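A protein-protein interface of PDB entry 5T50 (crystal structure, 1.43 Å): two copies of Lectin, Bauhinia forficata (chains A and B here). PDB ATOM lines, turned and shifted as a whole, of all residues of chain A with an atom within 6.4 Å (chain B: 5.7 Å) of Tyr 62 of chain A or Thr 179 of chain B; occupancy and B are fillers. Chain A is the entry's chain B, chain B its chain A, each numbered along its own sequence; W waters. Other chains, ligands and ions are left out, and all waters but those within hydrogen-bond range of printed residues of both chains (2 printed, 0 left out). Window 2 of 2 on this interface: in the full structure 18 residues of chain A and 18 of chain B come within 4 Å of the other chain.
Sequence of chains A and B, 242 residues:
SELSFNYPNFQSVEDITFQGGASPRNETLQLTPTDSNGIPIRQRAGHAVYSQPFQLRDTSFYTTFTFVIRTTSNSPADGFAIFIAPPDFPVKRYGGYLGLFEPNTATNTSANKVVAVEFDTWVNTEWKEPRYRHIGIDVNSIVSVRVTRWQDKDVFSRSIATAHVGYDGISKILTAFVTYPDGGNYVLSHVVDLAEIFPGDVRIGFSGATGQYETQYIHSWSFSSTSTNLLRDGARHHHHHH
The side-chain amide nitrogen of Asn 185 of chain B lies within hydrogen-bond range of the side-chain hydroxyl of Ser 224 of chain A (2.8 Å).
The backbone carbonyl oxygen of Thr 162 of chain B sits at hydrogen-bond distance from the backbone NH of Thr 179 of chain B, at 2.9 Å. The backbone NH (N) of His 164 of chain B is in hydrogen-bond range of the backbone carbonyl oxygen (O) of Phe 177 of chain B. The backbone NH (N) of Tyr 62 of chain A sits at hydrogen-bond distance from the backbone carbonyl oxygen (O) of Ser 224 of chain A. A ring nitrogen (ND1) of His 164 of chain A sits at hydrogen-bond distance from the side-chain hydroxyl (OG1) of Thr 64 of chain A (3.4 Å). A ring nitrogen (ND1) of His 164 of chain A is in hydrogen-bond range of the side-chain hydroxyl of Tyr 62 of chain A (2.7 Å). The backbone carbonyl oxygen (O) of Phe 61 of chain A lies within hydrogen-bond range of the backbone NH (N) of Tyr 167 of chain A (2.8 Å).
Among the printed residues, merely in contact across the chains: Gly 166 of chain A with Phe 177 of chain B (3.4 Å), His 164 of chain A with His 164 of chain B (3.5 Å), Phe 61 of chain A with Val 187 of chain B (3.5 Å), Tyr 62 of chain A with Thr 179 of chain B (3.7 Å), Tyr 62 of chain A with Asn 185 of chain B (3.7 Å), His 164 of chain A with Phe 177 of chain B (3.7 Å), Tyr 62 of chain A with Phe 177 of chain B (3.8 Å), Tyr 62 of chain A with Val 187 of chain B (3.8 Å) and Tyr 167 of chain A with Val 187 of chain B (3.9 Å).
Tyr 62 of chain A touches just these residues of chain B: Phe 177, Thr 179, Asn 185 and Val 187. Of chain A, only Tyr 62 comes within 4 Å of Thr 179 of chain B. Of the printed residues of chain A, Asn 185 of chain B touches Tyr 62 (3.7 Å) and Ser 224 (2.8 Å). Printed residues of chain B within 4 Å of His 164 of chain A: His 164 and Phe 177. Printed residues of chain B within 4 Å of Phe 61 of chain A: Val 187. Printed residues of chain B within 4 Å of Gly 166 of chain A: Phe 177 (3.4 Å). Of the printed residues of chain A, Val 187 of chain B touches Phe 61, Tyr 62 and Tyr 167. Gly 184 of chain B touches none of the printed residues of chain A. The nearest residue of chain B that does not touch Tyr 62 of chain A is His 164 of chain B (4.5 Å).
Of the 14 printed residues of chain B, 5 touch a printed residue of chain A. Hydrophobic or aromatic side chains of chain B within 4 Å of the printed part of chain A: His 164, Phe 177 and Val 187. Among the printed residues, 10 pairs touch across the chains.
His 164 of chain B touches its own counterpart, His 164 of chain A.
Water W1 bridges O of Val 187 of chain B (2.6 Å) and OG of Ser 60 of chain A (3.0 Å). Water W2 bridges the side-chain hydroxyl of Ser 222 of chain A (2.7 Å) and the side-chain amide nitrogen of Asn 185 of chain B (3.5 Å).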
ATOM      1  N   SER A  60      24.100  33.251  12.284  1.00  0.00           N
ATOM      2  CA  SER A  60      23.749  31.832  12.135  1.00  0.00           C
ATOM      3  C   SER A  60      24.295  31.388  10.770  1.00  0.00           C
ATOM      4  O   SER A  60      24.461  32.211   9.849  1.00  0.00           O
ATOM      5  CB  SER A  60      22.243  31.603  12.175  1.00  0.00           C
ATOM      6  OG  SER A  60      21.721  31.944  13.419  1.00  0.00           O
ATOM      7  N   PHE A  61      24.516  30.099  10.621  1.00  0.00           N
ATOM      8  CA  PHE A  61      24.932  29.597   9.337  1.00  0.00           C
ATOM      9  C   PHE A  61      24.427  28.188   9.070  1.00  0.00           C
ATOM     10  O   PHE A  61      24.068  27.430  10.012  1.00  0.00           O
ATOM     11  CB  PHE A  61      26.469  29.677   9.161  1.00  0.00           C
ATOM     12  CG  PHE A  61      27.322  28.717  10.001  1.00  0.00           C
ATOM     13  CD1 PHE A  61      27.404  27.337   9.685  1.00  0.00           C
ATOM     14  CD2 PHE A  61      28.050  29.182  11.097  1.00  0.00           C
ATOM     15  CE1 PHE A  61      28.145  26.450  10.443  1.00  0.00           C
ATOM     16  CE2 PHE A  61      28.793  28.296  11.856  1.00  0.00           C
ATOM     17  CZ  PHE A  61      28.838  26.946  11.553  1.00  0.00           C
ATOM     18  N   TYR A  62      24.391  27.843   7.788  1.00  0.00           N
ATOM     19  CA  TYR A  62      24.036  26.509   7.315  1.00  0.00           C
ATOM     20  C   TYR A  62      25.057  26.126   6.239  1.00  0.00           C
ATOM     21  O   TYR A  62      25.393  26.935   5.408  1.00  0.00           O
ATOM     22  CB  TYR A  62      22.650  26.496   6.671  1.00  0.00           C
ATOM     23  CG  TYR A  62      22.327  25.212   5.967  1.00  0.00           C
ATOM     24  CD1 TYR A  62      21.888  24.046   6.670  1.00  0.00           C
ATOM     25  CD2 TYR A  62      22.441  25.122   4.577  1.00  0.00           C
ATOM     26  CE1 TYR A  62      21.683  22.859   6.019  1.00  0.00           C
ATOM     27  CE2 TYR A  62      22.212  23.914   3.914  1.00  0.00           C
ATOM     28  CZ  TYR A  62      21.813  22.778   4.583  1.00  0.00           C
ATOM     29  OH  TYR A  62      21.539  21.575   3.982  1.00  0.00           O
ATOM     30  N   THR A  63      25.588  24.946   6.371  1.00  0.00           N
ATOM     31  CA  THR A  63      26.501  24.430   5.313  1.00  0.00           C
ATOM     32  C   THR A  63      26.196  22.949   5.065  1.00  0.00           C
ATOM     33  O   THR A  63      25.793  22.179   5.996  1.00  0.00           O
ATOM     34  CB  THR A  63      27.976  24.685   5.680  1.00  0.00           C
ATOM     35  OG1 THR A  63      28.863  24.464   4.594  1.00  0.00           O
ATOM     36  CG2 THR A  63      28.475  23.881   6.861  1.00  0.00           C
ATOM     37  N   THR A  64      26.382  22.527   3.813  1.00  0.00           N
ATOM     38  CA  THR A  64      26.167  21.133   3.481  1.00  0.00           C
ATOM     39  C   THR A  64      27.248  20.725   2.488  1.00  0.00           C
ATOM     40  O   THR A  64      27.717  21.558   1.682  1.00  0.00           O
ATOM     41  CB  THR A  64      24.750  20.877   2.914  1.00  0.00           C
ATOM     42  OG1 THR A  64      24.520  19.496   2.701  1.00  0.00           O
ATOM     43  CG2 THR A  64      24.491  21.618   1.593  1.00  0.00           C
ATOM     44  N   ALA A 163      26.536  15.581   4.547  1.00  0.00           N
ATOM     45  CA  ALA A 163      26.502  16.200   5.853  1.00  0.00           C
ATOM     46  C   ALA A 163      25.839  17.555   5.753  1.00  0.00           C
ATOM     47  O   ALA A 163      25.991  18.308   4.762  1.00  0.00           O
ATOM     48  CB  ALA A 163      27.914  16.364   6.426  1.00  0.00           C
ATOM     49  N   HIS A 164      25.141  17.861   6.829  1.00  0.00           N
ATOM     50  CA  HIS A 164      24.493  19.151   7.024  1.00  0.00           C
ATOM     51  C   HIS A 164      24.996  19.678   8.361  1.00  0.00           C
ATOM     52  O   HIS A 164      24.842  18.974   9.364  1.00  0.00           O
ATOM     53  CB  HIS A 164      22.968  19.035   7.122  1.00  0.00           C
ATOM     54  CG  HIS A 164      22.317  18.349   5.956  1.00  0.00           C
ATOM     55  ND1 HIS A 164      21.903  19.016   4.820  1.00  0.00           N
ATOM     56  CD2 HIS A 164      22.095  17.041   5.712  1.00  0.00           C
ATOM     57  CE1 HIS A 164      21.414  18.137   3.957  1.00  0.00           C
ATOM     58  NE2 HIS A 164      21.481  16.946   4.494  1.00  0.00           N
ATOM     59  N   VAL A 165      25.600  20.862   8.391  1.00  0.00           N
ATOM     60  CA  VAL A 165      26.060  21.416   9.630  1.00  0.00           C
ATOM     61  C   VAL A 165      25.514  22.826   9.779  1.00  0.00           C
ATOM     62  O   VAL A 165      25.599  23.643   8.862  1.00  0.00           O
ATOM     63  CB  VAL A 165      27.616  21.417   9.713  1.00  0.00           C
ATOM     64  CG1 VAL A 165      28.092  22.037  11.006  1.00  0.00           C
ATOM     65  CG2 VAL A 165      28.167  20.021   9.538  1.00  0.00           C
ATOM     66  N   GLY A 166      24.813  23.064  10.894  1.00  0.00           N
ATOM     67  CA  GLY A 166      24.253  24.370  11.124  1.00  0.00           C
ATOM     68  C   GLY A 166      24.558  24.943  12.481  1.00  0.00           C
ATOM     69  O   GLY A 166      24.806  24.196  13.445  1.00  0.00           O
ATOM     70  N   TYR A 167      24.489  26.272  12.553  1.00  0.00           N
ATOM     71  CA  TYR A 167      24.685  26.943  13.810  1.00  0.00           C
ATOM     72  C   TYR A 167      23.601  27.973  13.978  1.00  0.00           C
ATOM     73  O   TYR A 167      23.429  28.884  13.166  1.00  0.00           O
ATOM     74  CB  TYR A 167      26.043  27.649  13.867  1.00  0.00           C
ATOM     75  CG  TYR A 167      26.346  28.298  15.167  1.00  0.00           C
ATOM     76  CD1 TYR A 167      26.479  27.559  16.298  1.00  0.00           C
ATOM     77  CD2 TYR A 167      26.443  29.709  15.280  1.00  0.00           C
ATOM     78  CE1 TYR A 167      26.772  28.197  17.508  1.00  0.00           C
ATOM     79  CE2 TYR A 167      26.665  30.326  16.492  1.00  0.00           C
ATOM     80  CZ  TYR A 167      26.875  29.561  17.606  1.00  0.00           C
ATOM     81  OH  TYR A 167      27.117  30.158  18.846  1.00  0.00           O
ATOM     82  N   SER A 222      28.130  23.775  -0.136  1.00  0.00           N
ATOM     83  CA  SER A 222      27.513  25.071  -0.138  1.00  0.00           C
ATOM     84  C   SER A 222      27.419  25.646   1.290  1.00  0.00           C
ATOM     85  O   SER A 222      27.476  24.854   2.261  1.00  0.00           O
ATOM     86  CB  SER A 222      26.179  25.118  -0.892  1.00  0.00           C
ATOM     87  OG  SER A 222      25.255  24.299  -0.229  1.00  0.00           O
ATOM     88  N   PHE A 223      27.266  26.949   1.394  1.00  0.00           N
ATOM     89  CA  PHE A 223      27.332  27.656   2.702  1.00  0.00           C
ATOM     90  C   PHE A 223      26.516  28.889   2.602  1.00  0.00           C
ATOM     91  O   PHE A 223      26.598  29.597   1.611  1.00  0.00           O
ATOM     92  CB  PHE A 223      28.771  27.985   3.030  1.00  0.00           C
ATOM     93  CG  PHE A 223      28.968  28.795   4.303  1.00  0.00           C
ATOM     94  CD1 PHE A 223      28.851  30.169   4.344  1.00  0.00           C
ATOM     95  CD2 PHE A 223      29.417  28.156   5.476  1.00  0.00           C
ATOM     96  CE1 PHE A 223      29.037  30.852   5.522  1.00  0.00           C
ATOM     97  CE2 PHE A 223      29.568  28.836   6.637  1.00  0.00           C
ATOM     98  CZ  PHE A 223      29.432  30.193   6.665  1.00  0.00           C
ATOM     99  N   SER A 224      25.775  29.191   3.675  1.00  0.00           N
ATOM    100  CA  SER A 224      25.180  30.514   3.847  1.00  0.00           C
ATOM    101  C   SER A 224      25.186  30.952   5.293  1.00  0.00           C
ATOM    102  O   SER A 224      24.902  30.147   6.179  1.00  0.00           O
ATOM    103  CB  SER A 224      23.768  30.569   3.230  1.00  0.00           C
ATOM    104  OG  SER A 224      22.920  29.710   3.862  1.00  0.00           O
ATOM    105  N   SER A 225      25.517  32.201   5.558  1.00  0.00           N
ATOM    106  CA  SER A 225      25.464  32.763   6.874  1.00  0.00           C
ATOM    107  C   SER A 225      24.589  34.020   6.828  1.00  0.00           C
ATOM    108  O   SER A 225      24.563  34.743   5.828  1.00  0.00           O
ATOM    109  CB  SER A 225      26.801  33.105   7.467  1.00  0.00           C
ATOM    110  OG  SER A 225      27.522  34.033   6.684  1.00  0.00           O
ATOM    111  N   ILE B 160       9.946  23.298  -4.798  1.00  0.00           N
ATOM    112  CA  ILE B 160       9.987  22.160  -3.935  1.00  0.00           C
ATOM    113  C   ILE B 160      11.105  22.393  -2.934  1.00  0.00           C
ATOM    114  O   ILE B 160      12.313  22.279  -3.266  1.00  0.00           O
ATOM    115  CB  ILE B 160      10.106  20.806  -4.670  1.00  0.00           C
ATOM    116  CG1 ILE B 160       8.964  20.628  -5.667  1.00  0.00           C
ATOM    117  CG2 ILE B 160      10.169  19.675  -3.665  1.00  0.00           C
ATOM    118  CD1 ILE B 160       9.162  19.500  -6.605  1.00  0.00           C
ATOM    119  N   ALA B 161      10.742  22.712  -1.695  1.00  0.00           N
ATOM    120  CA  ALA B 161      11.679  23.002  -0.635  1.00  0.00           C
ATOM    121  C   ALA B 161      11.907  21.764   0.203  1.00  0.00           C
ATOM    122  O   ALA B 161      11.169  20.803   0.137  1.00  0.00           O
ATOM    123  CB  ALA B 161      11.129  24.130   0.244  1.00  0.00           C
ATOM    124  N   THR B 162      12.982  21.765   0.991  1.00  0.00           N
ATOM    125  CA  THR B 162      13.283  20.666   1.815  1.00  0.00           C
ATOM    126  C   THR B 162      13.391  21.086   3.302  1.00  0.00           C
ATOM    127  O   THR B 162      13.970  22.122   3.627  1.00  0.00           O
ATOM    128  CB  THR B 162      14.641  20.033   1.384  1.00  0.00           C
ATOM    129  OG1 THR B 162      14.535  19.546   0.052  1.00  0.00           O
ATOM    130  CG2 THR B 162      15.070  18.868   2.259  1.00  0.00           C
ATOM    131  N   ALA B 163      12.938  20.201   4.182  1.00  0.00           N
ATOM    132  CA  ALA B 163      13.162  20.354   5.630  1.00  0.00           C
ATOM    133  C   ALA B 163      13.890  19.137   6.144  1.00  0.00           C
ATOM    134  O   ALA B 163      13.605  18.007   5.684  1.00  0.00           O
ATOM    135  CB  ALA B 163      11.867  20.562   6.350  1.00  0.00           C
ATOM    136  N   HIS B 164      14.772  19.396   7.094  1.00  0.00           N
ATOM    137  CA  HIS B 164      15.440  18.384   7.850  1.00  0.00           C
ATOM    138  C   HIS B 164      15.150  18.672   9.334  1.00  0.00           C
ATOM    139  O   HIS B 164      15.430  19.781   9.796  1.00  0.00           O
ATOM    140  CB  HIS B 164      16.950  18.434   7.657  1.00  0.00           C
ATOM    141  CG  HIS B 164      17.389  18.412   6.243  1.00  0.00           C
ATOM    142  ND1 HIS B 164      17.661  17.241   5.604  1.00  0.00           N
ATOM    143  CD2 HIS B 164      17.543  19.401   5.343  1.00  0.00           C
ATOM    144  CE1 HIS B 164      18.025  17.523   4.356  1.00  0.00           C
ATOM    145  NE2 HIS B 164      17.958  18.823   4.169  1.00  0.00           N
ATOM    146  N   PHE B 177      16.523  22.397   9.855  1.00  0.00           N
ATOM    147  CA  PHE B 177      17.168  23.072   8.734  1.00  0.00           C
ATOM    148  C   PHE B 177      16.178  23.086   7.580  1.00  0.00           C
ATOM    149  O   PHE B 177      15.618  22.028   7.221  1.00  0.00           O
ATOM    150  CB  PHE B 177      18.429  22.359   8.239  1.00  0.00           C
ATOM    151  CG  PHE B 177      19.547  22.144   9.247  1.00  0.00           C
ATOM    152  CD1 PHE B 177      19.766  22.967  10.336  1.00  0.00           C
ATOM    153  CD2 PHE B 177      20.387  21.083   9.081  1.00  0.00           C
ATOM    154  CE1 PHE B 177      20.814  22.772  11.198  1.00  0.00           C
ATOM    155  CE2 PHE B 177      21.464  20.860   9.983  1.00  0.00           C
ATOM    156  CZ  PHE B 177      21.656  21.689  11.023  1.00  0.00           C
ATOM    157  N   VAL B 178      15.901  24.263   7.007  1.00  0.00           N
ATOM    158  CA  VAL B 178      14.978  24.334   5.885  1.00  0.00           C
ATOM    159  C   VAL B 178      15.764  25.008   4.741  1.00  0.00           C
ATOM    160  O   VAL B 178      16.438  26.013   4.965  1.00  0.00           O
ATOM    161  CB  VAL B 178      13.755  25.182   6.245  1.00  0.00           C
ATOM    162  CG1 VAL B 178      12.811  25.314   5.047  1.00  0.00           C
ATOM    163  CG2 VAL B 178      13.037  24.520   7.428  1.00  0.00           C
ATOM    164  N   THR B 179      15.671  24.447   3.550  1.00  0.00           N
ATOM    165  CA  THR B 179      16.456  24.878   2.395  1.00  0.00           C
ATOM    166  C   THR B 179      15.561  25.045   1.174  1.00  0.00           C
ATOM    167  O   THR B 179      14.642  24.224   0.941  1.00  0.00           O
ATOM    168  CB  THR B 179      17.587  23.877   2.069  1.00  0.00           C
ATOM    169  OG1 THR B 179      17.073  22.635   1.582  1.00  0.00           O
ATOM    170  CG2 THR B 179      18.502  23.643   3.265  1.00  0.00           C
ATOM    171  N   TYR B 180      15.818  26.095   0.409  1.00  0.00           N
ATOM    172  CA  TYR B 180      15.166  26.349  -0.869  1.00  0.00           C
ATOM    173  C   TYR B 180      16.217  26.331  -1.990  1.00  0.00           C
ATOM    174  O   TYR B 180      17.311  26.916  -1.819  1.00  0.00           O
ATOM    175  CB  TYR B 180      14.533  27.707  -0.865  1.00  0.00           C
ATOM    176  CG  TYR B 180      13.237  27.704  -0.126  1.00  0.00           C
ATOM    177  CD1 TYR B 180      13.203  27.772   1.285  1.00  0.00           C
ATOM    178  CD2 TYR B 180      12.027  27.660  -0.830  1.00  0.00           C
ATOM    179  CE1 TYR B 180      11.972  27.746   1.956  1.00  0.00           C
ATOM    180  CE2 TYR B 180      10.772  27.601  -0.189  1.00  0.00           C
ATOM    181  CZ  TYR B 180      10.760  27.661   1.203  1.00  0.00           C
ATOM    182  OH  TYR B 180       9.570  27.668   1.903  1.00  0.00           O
ATOM    183  N   PRO B 181      15.862  25.684  -3.115  1.00  0.00           N
ATOM    184  CA  PRO B 181      16.820  25.627  -4.221  1.00  0.00           C
ATOM    185  C   PRO B 181      17.063  27.047  -4.805  1.00  0.00           C
ATOM    186  O   PRO B 181      16.130  27.777  -5.173  1.00  0.00           O
ATOM    187  CB  PRO B 181      16.095  24.756  -5.241  1.00  0.00           C
ATOM    188  CG  PRO B 181      14.651  24.805  -4.958  1.00  0.00           C
ATOM    189  CD  PRO B 181      14.576  25.015  -3.456  1.00  0.00           C
ATOM    190  N   GLY B 184      16.631  30.771   0.171  1.00  0.00           N
ATOM    191  CA  GLY B 184      17.103  30.810   1.521  1.00  0.00           C
ATOM    192  C   GLY B 184      17.278  29.505   2.250  1.00  0.00           C
ATOM    193  O   GLY B 184      16.721  28.470   1.876  1.00  0.00           O
ATOM    194  N   ASN B 185      18.139  29.561   3.280  1.00  0.00           N
ATOM    195  CA  ASN B 185      18.345  28.462   4.216  1.00  0.00           C
ATOM    196  C   ASN B 185      18.063  29.017   5.585  1.00  0.00           C
ATOM    197  O   ASN B 185      18.338  30.199   5.944  1.00  0.00           O
ATOM    198  CB  ASN B 185      19.758  27.956   4.169  1.00  0.00           C
ATOM    199  CG  ASN B 185      20.139  27.444   2.815  1.00  0.00           C
ATOM    200  OD1 ASN B 185      19.448  26.671   2.157  1.00  0.00           O
ATOM    201  ND2 ASN B 185      21.330  27.881   2.394  1.00  0.00           N
ATOM    202  N   TYR B 186      17.491  28.144   6.433  1.00  0.00           N
ATOM    203  CA  TYR B 186      16.982  28.545   7.757  1.00  0.00           C
ATOM    204  C   TYR B 186      17.402  27.500   8.760  1.00  0.00           C
ATOM    205  O   TYR B 186      17.368  26.291   8.473  1.00  0.00           O
ATOM    206  CB  TYR B 186      15.430  28.594   7.740  1.00  0.00           C
ATOM    207  CG  TYR B 186      14.920  29.538   6.663  1.00  0.00           C
ATOM    208  CD1 TYR B 186      14.686  29.119   5.385  1.00  0.00           C
ATOM    209  CD2 TYR B 186      14.654  30.874   6.966  1.00  0.00           C
ATOM    210  CE1 TYR B 186      14.213  30.004   4.409  1.00  0.00           C
ATOM    211  CE2 TYR B 186      14.195  31.744   6.029  1.00  0.00           C
ATOM    212  CZ  TYR B 186      13.985  31.312   4.732  1.00  0.00           C
ATOM    213  OH  TYR B 186      13.489  32.213   3.810  1.00  0.00           O
ATOM    214  N   VAL B 187      17.860  27.962   9.907  1.00  0.00           N
ATOM    215  CA  VAL B 187      18.344  27.113  10.986  1.00  0.00           C
ATOM    216  C   VAL B 187      17.725  27.513  12.313  1.00  0.00           C
ATOM    217  O   VAL B 187      17.813  28.665  12.711  1.00  0.00           O
ATOM    218  CB  VAL B 187      19.886  27.226  11.125  1.00  0.00           C
ATOM    219  CG1 VAL B 187      20.392  26.443  12.318  1.00  0.00           C
ATOM    220  CG2 VAL B 187      20.608  26.802   9.883  1.00  0.00           C
HETATM  221  O   HOH W   1      18.961  31.044  12.812  1.00  0.00           O
HETATM  222  O   HOH W   2      22.985  25.469   0.515  1.00  0.00           O
